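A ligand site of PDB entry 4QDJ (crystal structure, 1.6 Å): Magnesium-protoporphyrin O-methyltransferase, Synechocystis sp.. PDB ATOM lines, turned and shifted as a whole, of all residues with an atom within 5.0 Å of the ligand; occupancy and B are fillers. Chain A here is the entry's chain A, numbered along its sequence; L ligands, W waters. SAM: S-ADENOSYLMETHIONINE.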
ATOM      1  N   LYS A   9      17.291 -38.512 -13.999  1.00  0.00           N
ATOM      2  CA  LYS A   9      17.056 -37.428 -14.948  1.00  0.00           C
ATOM      3  C   LYS A   9      15.781 -36.651 -14.632  1.00  0.00           C
ATOM      4  O   LYS A   9      15.756 -35.434 -14.731  1.00  0.00           O
ATOM      5  CB  LYS A   9      16.997 -37.968 -16.384  1.00  0.00           C
ATOM      6  CG  LYS A   9      18.338 -38.384 -16.947  1.00  0.00           C
ATOM      7  CD  LYS A   9      18.185 -38.937 -18.348  1.00  0.00           C
ATOM      8  CE  LYS A   9      19.523 -39.370 -18.915  1.00  0.00           C
ATOM      9  NZ  LYS A   9      19.378 -39.973 -20.273  1.00  0.00           N
ATOM     10  N   VAL A  12      16.308 -34.513 -11.432  1.00  0.00           N
ATOM     11  CA  VAL A  12      17.109 -33.343 -11.756  1.00  0.00           C
ATOM     12  C   VAL A  12      16.316 -32.336 -12.595  1.00  0.00           C
ATOM     13  O   VAL A  12      16.322 -31.141 -12.298  1.00  0.00           O
ATOM     14  CB  VAL A  12      18.419 -33.726 -12.468  1.00  0.00           C
ATOM     15  CG1 VAL A  12      19.181 -32.479 -12.872  1.00  0.00           C
ATOM     16  CG2 VAL A  12      19.262 -34.611 -11.572  1.00  0.00           C
ATOM     17  N   PHE A  16      15.273 -28.409 -11.492  1.00  0.00           N
ATOM     18  CA  PHE A  16      15.633 -27.211 -12.244  1.00  0.00           C
ATOM     19  C   PHE A  16      14.449 -26.553 -12.957  1.00  0.00           C
ATOM     20  O   PHE A  16      14.562 -25.460 -13.496  1.00  0.00           O
ATOM     21  CB  PHE A  16      16.768 -27.504 -13.227  1.00  0.00           C
ATOM     22  CG  PHE A  16      18.112 -27.617 -12.582  1.00  0.00           C
ATOM     23  CD1 PHE A  16      18.821 -26.476 -12.220  1.00  0.00           C
ATOM     24  CD2 PHE A  16      18.679 -28.852 -12.306  1.00  0.00           C
ATOM     25  CE1 PHE A  16      20.058 -26.569 -11.610  1.00  0.00           C
ATOM     26  CE2 PHE A  16      19.910 -28.954 -11.704  1.00  0.00           C
ATOM     27  CZ  PHE A  16      20.606 -27.813 -11.355  1.00  0.00           C
ATOM     28  N   TRP A  24      19.237 -21.216  -8.842  1.00  0.00           N
ATOM     29  CA  TRP A  24      20.376 -21.157  -9.761  1.00  0.00           C
ATOM     30  C   TRP A  24      20.344 -19.964 -10.712  1.00  0.00           C
ATOM     31  O   TRP A  24      21.390 -19.467 -11.127  1.00  0.00           O
ATOM     32  CB  TRP A  24      20.576 -22.491 -10.483  1.00  0.00           C
ATOM     33  CG  TRP A  24      21.125 -23.522  -9.551  1.00  0.00           C
ATOM     34  CD1 TRP A  24      20.411 -24.468  -8.858  1.00  0.00           C
ATOM     35  CD2 TRP A  24      22.487 -23.681  -9.146  1.00  0.00           C
ATOM     36  NE1 TRP A  24      21.252 -25.224  -8.081  1.00  0.00           N
ATOM     37  CE2 TRP A  24      22.532 -24.761  -8.238  1.00  0.00           C
ATOM     38  CE3 TRP A  24      23.682 -23.029  -9.480  1.00  0.00           C
ATOM     39  CZ2 TRP A  24      23.731 -25.197  -7.658  1.00  0.00           C
ATOM     40  CZ3 TRP A  24      24.860 -23.471  -8.912  1.00  0.00           C
ATOM     41  CH2 TRP A  24      24.878 -24.545  -8.011  1.00  0.00           C
ATOM     42  N   TYR A  28      23.629 -17.779 -10.776  1.00  0.00           N
ATOM     43  CA  TYR A  28      24.229 -17.509 -12.071  1.00  0.00           C
ATOM     44  C   TYR A  28      23.922 -16.118 -12.600  1.00  0.00           C
ATOM     45  O   TYR A  28      24.403 -15.729 -13.668  1.00  0.00           O
ATOM     46  CB  TYR A  28      23.761 -18.535 -13.098  1.00  0.00           C
ATOM     47  CG  TYR A  28      24.288 -19.936 -12.902  1.00  0.00           C
ATOM     48  CD1 TYR A  28      25.436 -20.175 -12.148  1.00  0.00           C
ATOM     49  CD2 TYR A  28      23.651 -21.028 -13.480  1.00  0.00           C
ATOM     50  CE1 TYR A  28      25.929 -21.460 -11.983  1.00  0.00           C
ATOM     51  CE2 TYR A  28      24.130 -22.305 -13.310  1.00  0.00           C
ATOM     52  CZ  TYR A  28      25.263 -22.522 -12.567  1.00  0.00           C
ATOM     53  OH  TYR A  28      25.742 -23.799 -12.396  1.00  0.00           O
ATOM     54  N   HIS A  44      32.057 -20.653 -10.151  1.00  0.00           N
ATOM     55  CA  HIS A  44      31.481 -21.030 -11.427  1.00  0.00           C
ATOM     56  C   HIS A  44      31.892 -20.053 -12.528  1.00  0.00           C
ATOM     57  O   HIS A  44      32.166 -20.468 -13.659  1.00  0.00           O
ATOM     58  CB  HIS A  44      29.957 -21.108 -11.324  1.00  0.00           C
ATOM     59  CG  HIS A  44      29.262 -21.240 -12.653  1.00  0.00           C
ATOM     60  ND1 HIS A  44      28.632 -20.183 -13.259  1.00  0.00           N
ATOM     61  CD2 HIS A  44      29.116 -22.299 -13.475  1.00  0.00           C
ATOM     62  CE1 HIS A  44      28.124 -20.581 -14.407  1.00  0.00           C
ATOM     63  NE2 HIS A  44      28.399 -21.869 -14.569  1.00  0.00           N
ATOM     64  N   VAL A  48      33.804 -20.975 -16.103  1.00  0.00           N
ATOM     65  CA  VAL A  48      33.361 -20.467 -17.394  1.00  0.00           C
ATOM     66  C   VAL A  48      34.466 -19.663 -18.078  1.00  0.00           C
ATOM     67  O   VAL A  48      34.797 -19.921 -19.242  1.00  0.00           O
ATOM     68  CB  VAL A  48      32.095 -19.608 -17.252  1.00  0.00           C
ATOM     69  CG1 VAL A  48      31.793 -18.881 -18.557  1.00  0.00           C
ATOM     70  CG2 VAL A  48      30.913 -20.474 -16.828  1.00  0.00           C
ATOM     71  N   ASP A  68      26.968 -27.031 -26.361  1.00  0.00           N
ATOM     72  CA  ASP A  68      26.974 -26.762 -24.920  1.00  0.00           C
ATOM     73  C   ASP A  68      25.859 -27.595 -24.281  1.00  0.00           C
ATOM     74  O   ASP A  68      24.703 -27.174 -24.260  1.00  0.00           O
ATOM     75  CB  ASP A  68      26.764 -25.270 -24.657  1.00  0.00           C
ATOM     76  CG  ASP A  68      26.943 -24.880 -23.207  1.00  0.00           C
ATOM     77  OD1 ASP A  68      27.317 -25.736 -22.374  1.00  0.00           O
ATOM     78  OD2 ASP A  68      26.726 -23.693 -22.886  1.00  0.00           O
ATOM     79  N   ALA A  69      26.214 -28.772 -23.788  1.00  0.00           N
ATOM     80  CA  ALA A  69      25.249 -29.724 -23.263  1.00  0.00           C
ATOM     81  C   ALA A  69      24.992 -29.513 -21.774  1.00  0.00           C
ATOM     82  O   ALA A  69      25.910 -29.582 -20.961  1.00  0.00           O
ATOM     83  CB  ALA A  69      25.731 -31.147 -23.512  1.00  0.00           C
ATOM     84  N   GLY A  70      23.732 -29.269 -21.423  1.00  0.00           N
ATOM     85  CA  GLY A  70      23.375 -28.879 -20.066  1.00  0.00           C
ATOM     86  C   GLY A  70      23.747 -27.424 -19.840  1.00  0.00           C
ATOM     87  O   GLY A  70      24.396 -27.074 -18.858  1.00  0.00           O
ATOM     88  N   CYS A  71      23.314 -26.579 -20.776  1.00  0.00           N
ATOM     89  CA  CYS A  71      23.791 -25.190 -20.857  1.00  0.00           C
ATOM     90  C   CYS A  71      23.287 -24.265 -19.752  1.00  0.00           C
ATOM     91  O   CYS A  71      23.771 -23.143 -19.614  1.00  0.00           O
ATOM     92  CB  CYS A  71      23.436 -24.602 -22.222  1.00  0.00           C
ATOM     93  SG  CYS A  71      21.656 -24.422 -22.514  1.00  0.00           S
ATOM     94  N   GLY A  72      22.317 -24.724 -18.971  1.00  0.00           N
ATOM     95  CA  GLY A  72      21.767 -23.905 -17.895  1.00  0.00           C
ATOM     96  C   GLY A  72      21.155 -22.627 -18.436  1.00  0.00           C
ATOM     97  O   GLY A  72      20.375 -22.657 -19.384  1.00  0.00           O
ATOM     98  N   SER A  75      25.396 -19.410 -19.310  1.00  0.00           N
ATOM     99  CA  SER A  75      26.586 -18.751 -18.764  1.00  0.00           C
ATOM    100  C   SER A  75      27.822 -18.943 -19.642  1.00  0.00           C
ATOM    101  O   SER A  75      28.664 -18.058 -19.723  1.00  0.00           O
ATOM    102  CB  SER A  75      26.879 -19.264 -17.353  1.00  0.00           C
ATOM    103  OG  SER A  75      25.800 -18.963 -16.473  1.00  0.00           O
ATOM    104  N   LEU A  76      27.920 -20.104 -20.276  1.00  0.00           N
ATOM    105  CA  LEU A  76      29.019 -20.364 -21.201  1.00  0.00           C
ATOM    106  C   LEU A  76      28.618 -20.074 -22.648  1.00  0.00           C
ATOM    107  O   LEU A  76      29.407 -19.517 -23.421  1.00  0.00           O
ATOM    108  CB  LEU A  76      29.514 -21.799 -21.084  1.00  0.00           C
ATOM    109  CG  LEU A  76      30.626 -22.192 -22.062  1.00  0.00           C
ATOM    110  CD1 LEU A  76      31.908 -21.446 -21.756  1.00  0.00           C
ATOM    111  CD2 LEU A  76      30.850 -23.694 -22.057  1.00  0.00           C
ATOM    112  N   SER A  90      21.851 -26.780 -25.120  1.00  0.00           N
ATOM    113  CA  SER A  90      20.671 -27.558 -24.775  1.00  0.00           C
ATOM    114  C   SER A  90      20.670 -27.885 -23.299  1.00  0.00           C
ATOM    115  O   SER A  90      21.729 -27.966 -22.678  1.00  0.00           O
ATOM    116  CB  SER A  90      20.604 -28.840 -25.603  1.00  0.00           C
ATOM    117  OG  SER A  90      21.781 -29.603 -25.448  1.00  0.00           O
ATOM    118  N   ASP A  91      19.478 -28.042 -22.741  1.00  0.00           N
ATOM    119  CA  ASP A  91      19.330 -28.361 -21.324  1.00  0.00           C
ATOM    120  C   ASP A  91      18.051 -29.148 -21.132  1.00  0.00           C
ATOM    121  O   ASP A  91      17.081 -28.954 -21.862  1.00  0.00           O
ATOM    122  CB  ASP A  91      19.298 -27.068 -20.505  1.00  0.00           C
ATOM    123  CG  ASP A  91      19.574 -27.317 -19.029  1.00  0.00           C
ATOM    124  OD1 ASP A  91      18.667 -27.816 -18.330  1.00  0.00           O
ATOM    125  OD2 ASP A  91      20.691 -26.990 -18.577  1.00  0.00           O
ATOM    126  N   ILE A  92      18.043 -30.042 -20.145  1.00  0.00           N
ATOM    127  CA  ILE A  92      16.881 -30.886 -19.902  1.00  0.00           C
ATOM    128  C   ILE A  92      15.731 -30.068 -19.299  1.00  0.00           C
ATOM    129  O   ILE A  92      14.570 -30.466 -19.358  1.00  0.00           O
ATOM    130  CB  ILE A  92      17.243 -32.081 -18.997  1.00  0.00           C
ATOM    131  CG1 ILE A  92      16.191 -33.189 -19.108  1.00  0.00           C
ATOM    132  CG2 ILE A  92      17.437 -31.635 -17.556  1.00  0.00           C
ATOM    133  CD1 ILE A  92      16.576 -34.471 -18.404  1.00  0.00           C
ATOM    134  N   SER A  93      16.070 -28.916 -18.726  1.00  0.00           N
ATOM    135  CA  SER A  93      15.087 -28.061 -18.070  1.00  0.00           C
ATOM    136  C   SER A  93      14.601 -26.934 -18.988  1.00  0.00           C
ATOM    137  O   SER A  93      15.376 -26.079 -19.404  1.00  0.00           O
ATOM    138  CB  SER A  93      15.685 -27.456 -16.796  1.00  0.00           C
ATOM    139  OG  SER A  93      14.944 -26.327 -16.368  1.00  0.00           O
ATOM    140  N   MET A  96      15.293 -23.396 -17.449  1.00  0.00           N
ATOM    141  CA  MET A  96      16.663 -22.933 -17.636  1.00  0.00           C
ATOM    142  C   MET A  96      16.892 -22.475 -19.076  1.00  0.00           C
ATOM    143  O   MET A  96      17.455 -21.402 -19.308  1.00  0.00           O
ATOM    144  CB  MET A  96      17.679 -24.008 -17.225  1.00  0.00           C
ATOM    145  CG  MET A  96      17.583 -24.434 -15.756  1.00  0.00           C
ATOM    146  SD  MET A  96      18.169 -23.188 -14.583  1.00  0.00           S
ATOM    147  CE  MET A  96      19.941 -23.446 -14.664  1.00  0.00           C
ATOM    148  N   GLN A 119      16.259 -30.447 -24.182  1.00  0.00           N
ATOM    149  CA  GLN A 119      16.535 -31.841 -24.507  1.00  0.00           C
ATOM    150  C   GLN A 119      17.507 -32.472 -23.511  1.00  0.00           C
ATOM    151  O   GLN A 119      18.428 -31.815 -23.027  1.00  0.00           O
ATOM    152  CB  GLN A 119      17.101 -31.957 -25.923  1.00  0.00           C
ATOM    153  CG  GLN A 119      17.306 -33.391 -26.418  1.00  0.00           C
ATOM    154  CD  GLN A 119      16.034 -34.197 -26.425  1.00  0.00           C
ATOM    155  OE1 GLN A 119      15.606 -34.728 -25.400  1.00  0.00           O
ATOM    156  NE2 GLN A 119      15.409 -34.310 -27.598  1.00  0.00           N
ATOM    157  N   ASP A 120      17.267 -33.739 -23.193  1.00  0.00           N
ATOM    158  CA  ASP A 120      18.222 -34.558 -22.449  1.00  0.00           C
ATOM    159  C   ASP A 120      19.457 -34.746 -23.318  1.00  0.00           C
ATOM    160  O   ASP A 120      19.341 -35.088 -24.494  1.00  0.00           O
ATOM    161  CB  ASP A 120      17.560 -35.912 -22.127  1.00  0.00           C
ATOM    162  CG  ASP A 120      18.535 -36.933 -21.560  1.00  0.00           C
ATOM    163  OD1 ASP A 120      19.584 -36.554 -20.997  1.00  0.00           O
ATOM    164  OD2 ASP A 120      18.217 -38.140 -21.660  1.00  0.00           O
ATOM    165  N   LEU A 121      20.635 -34.494 -22.760  1.00  0.00           N
ATOM    166  CA  LEU A 121      21.871 -34.549 -23.541  1.00  0.00           C
ATOM    167  C   LEU A 121      22.116 -35.927 -24.151  1.00  0.00           C
ATOM    168  O   LEU A 121      22.781 -36.044 -25.180  1.00  0.00           O
ATOM    169  CB  LEU A 121      23.079 -34.089 -22.704  1.00  0.00           C
ATOM    170  CG  LEU A 121      23.510 -34.868 -21.457  1.00  0.00           C
ATOM    171  CD1 LEU A 121      24.403 -36.051 -21.796  1.00  0.00           C
ATOM    172  CD2 LEU A 121      24.205 -33.927 -20.491  1.00  0.00           C
ATOM    173  N   LEU A 134      29.724 -28.693 -18.699  1.00  0.00           N
ATOM    174  CA  LEU A 134      30.267 -28.138 -17.457  1.00  0.00           C
ATOM    175  C   LEU A 134      29.294 -28.253 -16.293  1.00  0.00           C
ATOM    176  O   LEU A 134      28.137 -27.846 -16.397  1.00  0.00           O
ATOM    177  CB  LEU A 134      30.630 -26.662 -17.634  1.00  0.00           C
ATOM    178  CG  LEU A 134      31.659 -26.286 -18.700  1.00  0.00           C
ATOM    179  CD1 LEU A 134      31.967 -24.797 -18.607  1.00  0.00           C
ATOM    180  CD2 LEU A 134      32.921 -27.120 -18.558  1.00  0.00           C
ATOM    181  N   ASP A 135      29.780 -28.803 -15.185  1.00  0.00           N
ATOM    182  CA  ASP A 135      29.019 -28.873 -13.931  1.00  0.00           C
ATOM    183  C   ASP A 135      27.653 -29.532 -14.089  1.00  0.00           C
ATOM    184  O   ASP A 135      26.673 -29.097 -13.490  1.00  0.00           O
ATOM    185  CB  ASP A 135      28.887 -27.486 -13.286  1.00  0.00           C
ATOM    186  CG  ASP A 135      30.214 -26.885 -12.870  1.00  0.00           C
ATOM    187  OD1 ASP A 135      31.256 -27.585 -12.958  1.00  0.00           O
ATOM    188  OD2 ASP A 135      30.229 -25.709 -12.443  1.00  0.00           O
ATOM    189  N   VAL A 136      27.596 -30.566 -14.918  1.00  0.00           N
ATOM    190  CA  VAL A 136      26.367 -31.315 -15.139  1.00  0.00           C
ATOM    191  C   VAL A 136      26.504 -32.727 -14.573  1.00  0.00           C
ATOM    192  O   VAL A 136      25.585 -33.255 -13.941  1.00  0.00           O
ATOM    193  CB  VAL A 136      26.018 -31.391 -16.646  1.00  0.00           C
ATOM    194  CG1 VAL A 136      24.822 -32.300 -16.872  1.00  0.00           C
ATOM    195  CG2 VAL A 136      25.769 -30.002 -17.198  1.00  0.00           C
ATOM    196  N   HIS A 139      25.470 -34.314 -11.080  1.00  0.00           N
ATOM    197  CA  HIS A 139      24.114 -34.739 -10.732  1.00  0.00           C
ATOM    198  C   HIS A 139      23.856 -36.229 -10.937  1.00  0.00           C
ATOM    199  O   HIS A 139      22.755 -36.714 -10.710  1.00  0.00           O
ATOM    200  CB  HIS A 139      23.087 -33.942 -11.532  1.00  0.00           C
ATOM    201  CG  HIS A 139      23.138 -32.468 -11.288  1.00  0.00           C
ATOM    202  ND1 HIS A 139      22.758 -31.895 -10.096  1.00  0.00           N
ATOM    203  CD2 HIS A 139      23.545 -31.440 -12.082  1.00  0.00           C
ATOM    204  CE1 HIS A 139      22.915 -30.588 -10.160  1.00  0.00           C
ATOM    205  NE2 HIS A 139      23.392 -30.291 -11.354  1.00  0.00           N
ATOM    206  N   TYR A 140      24.891 -36.963 -11.361  1.00  0.00           N
ATOM    207  CA  TYR A 140      24.727 -38.372 -11.694  1.00  0.00           C
ATOM    208  C   TYR A 140      25.848 -39.244 -11.132  1.00  0.00           C
ATOM    209  O   TYR A 140      26.986 -38.801 -11.030  1.00  0.00           O
ATOM    210  CB  TYR A 140      24.646 -38.538 -13.221  1.00  0.00           C
ATOM    211  CG  TYR A 140      23.507 -37.764 -13.832  1.00  0.00           C
ATOM    212  CD1 TYR A 140      22.224 -38.288 -13.869  1.00  0.00           C
ATOM    213  CD2 TYR A 140      23.708 -36.495 -14.354  1.00  0.00           C
ATOM    214  CE1 TYR A 140      21.176 -37.585 -14.427  1.00  0.00           C
ATOM    215  CE2 TYR A 140      22.672 -35.775 -14.917  1.00  0.00           C
ATOM    216  CZ  TYR A 140      21.403 -36.322 -14.942  1.00  0.00           C
ATOM    217  OH  TYR A 140      20.364 -35.614 -15.500  1.00  0.00           O
ATOM    218  N   MET A 148      26.796 -41.050 -20.223  1.00  0.00           N
ATOM    219  CA  MET A 148      26.636 -39.687 -20.707  1.00  0.00           C
ATOM    220  C   MET A 148      27.872 -39.206 -21.457  1.00  0.00           C
ATOM    221  O   MET A 148      27.773 -38.626 -22.538  1.00  0.00           O
ATOM    222  CB  MET A 148      26.310 -38.744 -19.550  1.00  0.00           C
ATOM    223  CG  MET A 148      24.921 -38.956 -18.966  1.00  0.00           C
ATOM    224  SD  MET A 148      24.638 -38.039 -17.432  1.00  0.00           S
ATOM    225  CE  MET A 148      24.891 -36.355 -17.973  1.00  0.00           C
HETATM  226  N   SAM L   1      26.554 -26.008 -17.697  1.00  0.00           N
HETATM  227  CA  SAM L   1      25.885 -24.843 -17.131  1.00  0.00           C
HETATM  228  C   SAM L   1      26.891 -23.891 -16.515  1.00  0.00           C
HETATM  229  O   SAM L   1      27.975 -24.288 -16.099  1.00  0.00           O
HETATM  230  OXT SAM L   1      26.636 -22.690 -16.424  1.00  0.00           O
HETATM  231  CB  SAM L   1      24.805 -25.239 -16.119  1.00  0.00           C
HETATM  232  CG  SAM L   1      25.257 -26.061 -14.906  1.00  0.00           C
HETATM  233  SD  SAM L   1      23.886 -26.367 -13.747  1.00  0.00           S
HETATM  234  CE  SAM L   1      24.787 -26.779 -12.229  1.00  0.00           C
HETATM  235  C5' SAM L   1      23.389 -28.027 -14.257  1.00  0.00           C
HETATM  236  C4' SAM L   1      22.457 -27.986 -15.464  1.00  0.00           C
HETATM  237  O4' SAM L   1      22.496 -29.247 -16.099  1.00  0.00           O
HETATM  238  C3' SAM L   1      21.011 -27.715 -15.088  1.00  0.00           C
HETATM  239  O3' SAM L   1      20.537 -26.631 -15.855  1.00  0.00           O
HETATM  240  C2' SAM L   1      20.276 -28.976 -15.481  1.00  0.00           C
HETATM  241  O2' SAM L   1      18.978 -28.703 -15.988  1.00  0.00           O
HETATM  242  C1' SAM L   1      21.197 -29.553 -16.544  1.00  0.00           C
HETATM  243  N9  SAM L   1      21.054 -31.000 -16.726  1.00  0.00           N
HETATM  244  C8  SAM L   1      21.005 -31.967 -15.760  1.00  0.00           C
HETATM  245  N7  SAM L   1      20.864 -33.166 -16.360  1.00  0.00           N
HETATM  246  C5  SAM L   1      20.829 -32.981 -17.696  1.00  0.00           C
HETATM  247  C6  SAM L   1      20.696 -33.852 -18.768  1.00  0.00           C
HETATM  248  N6  SAM L   1      20.585 -35.159 -18.555  1.00  0.00           N
HETATM  249  N1  SAM L   1      20.696 -33.354 -20.052  1.00  0.00           N
HETATM  250  C2  SAM L   1      20.813 -31.997 -20.273  1.00  0.00           C
HETATM  251  N3  SAM L   1      20.937 -31.131 -19.201  1.00  0.00           N
HETATM  252  C4  SAM L   1      20.952 -31.619 -17.940  1.00  0.00           C
HETATM  253  O   HOH W   1      24.351 -21.237 -16.965  1.00  0.00           O
HETATM  254  O   HOH W   2      27.585 -27.466 -20.195  1.00  0.00           O
HETATM  255  O   HOH W   3      27.915 -24.524 -19.788  1.00  0.00           O
HETATM  256  O   HOH W   4      21.221 -31.246 -23.367  1.00  0.00           O
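The side-chain carboxylate of Asp 91 lies within hydrogen-bond range of the backbone NH of Ser 93.
The backbone NH (N) of Gly 72 is in hydrogen-bond range of the side-chain carboxylate (OD2) of Asp 91 (2.8 Å).
The backbone carbonyl oxygen (O) of Asp 91 sits at hydrogen-bond distance from the backbone NH (N) of Gln 119 (2.9 Å).
O of Ser 90 lies within hydrogen-bond range of N of Gly 70 (2.7 Å).
The side-chain amino group (NZ) of Lys 9 is in salt-bridge range of the side-chain carboxylate (OD2) of Asp 120 (2.6 Å).
N of Ile 92 is in hydrogen-bond range of O of Gln 119, 3.4 Å away.
N of Met 96 lies within hydrogen-bond range of OG of Ser 93, 3.1 Å away.
The backbone carbonyl oxygen of Phe 16 is in hydrogen-bond range of the side-chain hydroxyl of Ser 93 (3.0 Å).
OH of Tyr 28 sits close to SD of the ligand, at 3.4 Å.
Residues that only touch the ligand: Val 12 (3.5 Å), Phe 16 (3.6 Å), Cys 71 (3.7 Å), Gly 72 (3.6 Å), Ser 75 (3.6 Å), Ser 93 (3.6 Å), Met 96 (3.5 Å), Gln 119 (3.6 Å), Asp 135 (3.2 Å), Val 136 (3.5 Å) and His 139 (3.7 Å).
Hydrophobic or aromatic side chains within 4 Å of the ligand: Val 12, Phe 16, His 44, Ile 92, Met 96, Leu 121, Leu 134, Val 136 and Tyr 140.
20 residues have an atom within 4 Å of the ligand: Val 12, Phe 16, Tyr 28, His 44, Gly 70, Cys 71, Gly 72, Ser 75, Asp 91, Ile 92, Ser 93, Met 96, Gln 119, Asp 120, Leu 121, Leu 134, Asp 135, Val 136, His 139 and Tyr 140.
The nearest printed residue that does not touch the ligand is Lys 9 (4.2 Å).
OD1 of Asp 91 is in hydrogen-bond range of O2' of the ligand, 2.5 Å away.
A nitrogen (N7) of the ligand is in hydrogen-bond range of the side-chain hydroxyl of Tyr 140, at 2.6 Å.
A nitrogen (N) of the ligand is in hydrogen-bond range of the backbone carbonyl oxygen (O) of Gly 70.
NE2 of His 44 sits at hydrogen-bond distance from OXT of the ligand (2.7 Å).
A nitrogen (N) of the ligand is in hydrogen-bond range of the backbone carbonyl oxygen (O) of Leu 134 (2.8 Å).
The backbone NH of Leu 121 is in hydrogen-bond range of a nitrogen (N1) of the ligand, at 2.9 Å.
A nitrogen (N6) of the ligand lies within hydrogen-bond range of the side-chain carboxylate of Asp 120 (3.0 Å).
The backbone NH of Ile 92 sits at hydrogen-bond distance from a nitrogen (N3) of the ligand.
Water W1 lies within hydrogen-bond range of OG of Ser 75, OXT of the ligand and O of Cys 71.
Water W3 lies within hydrogen-bond range of a nitrogen (N) of the ligand and the side-chain carboxylate (OD1) of Asp 68.
Water W4 lies within hydrogen-bond range of OG of Ser 90 (2.7 Å), O of Gln 119 (2.9 Å) and N of Leu 121 (3.4 Å).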
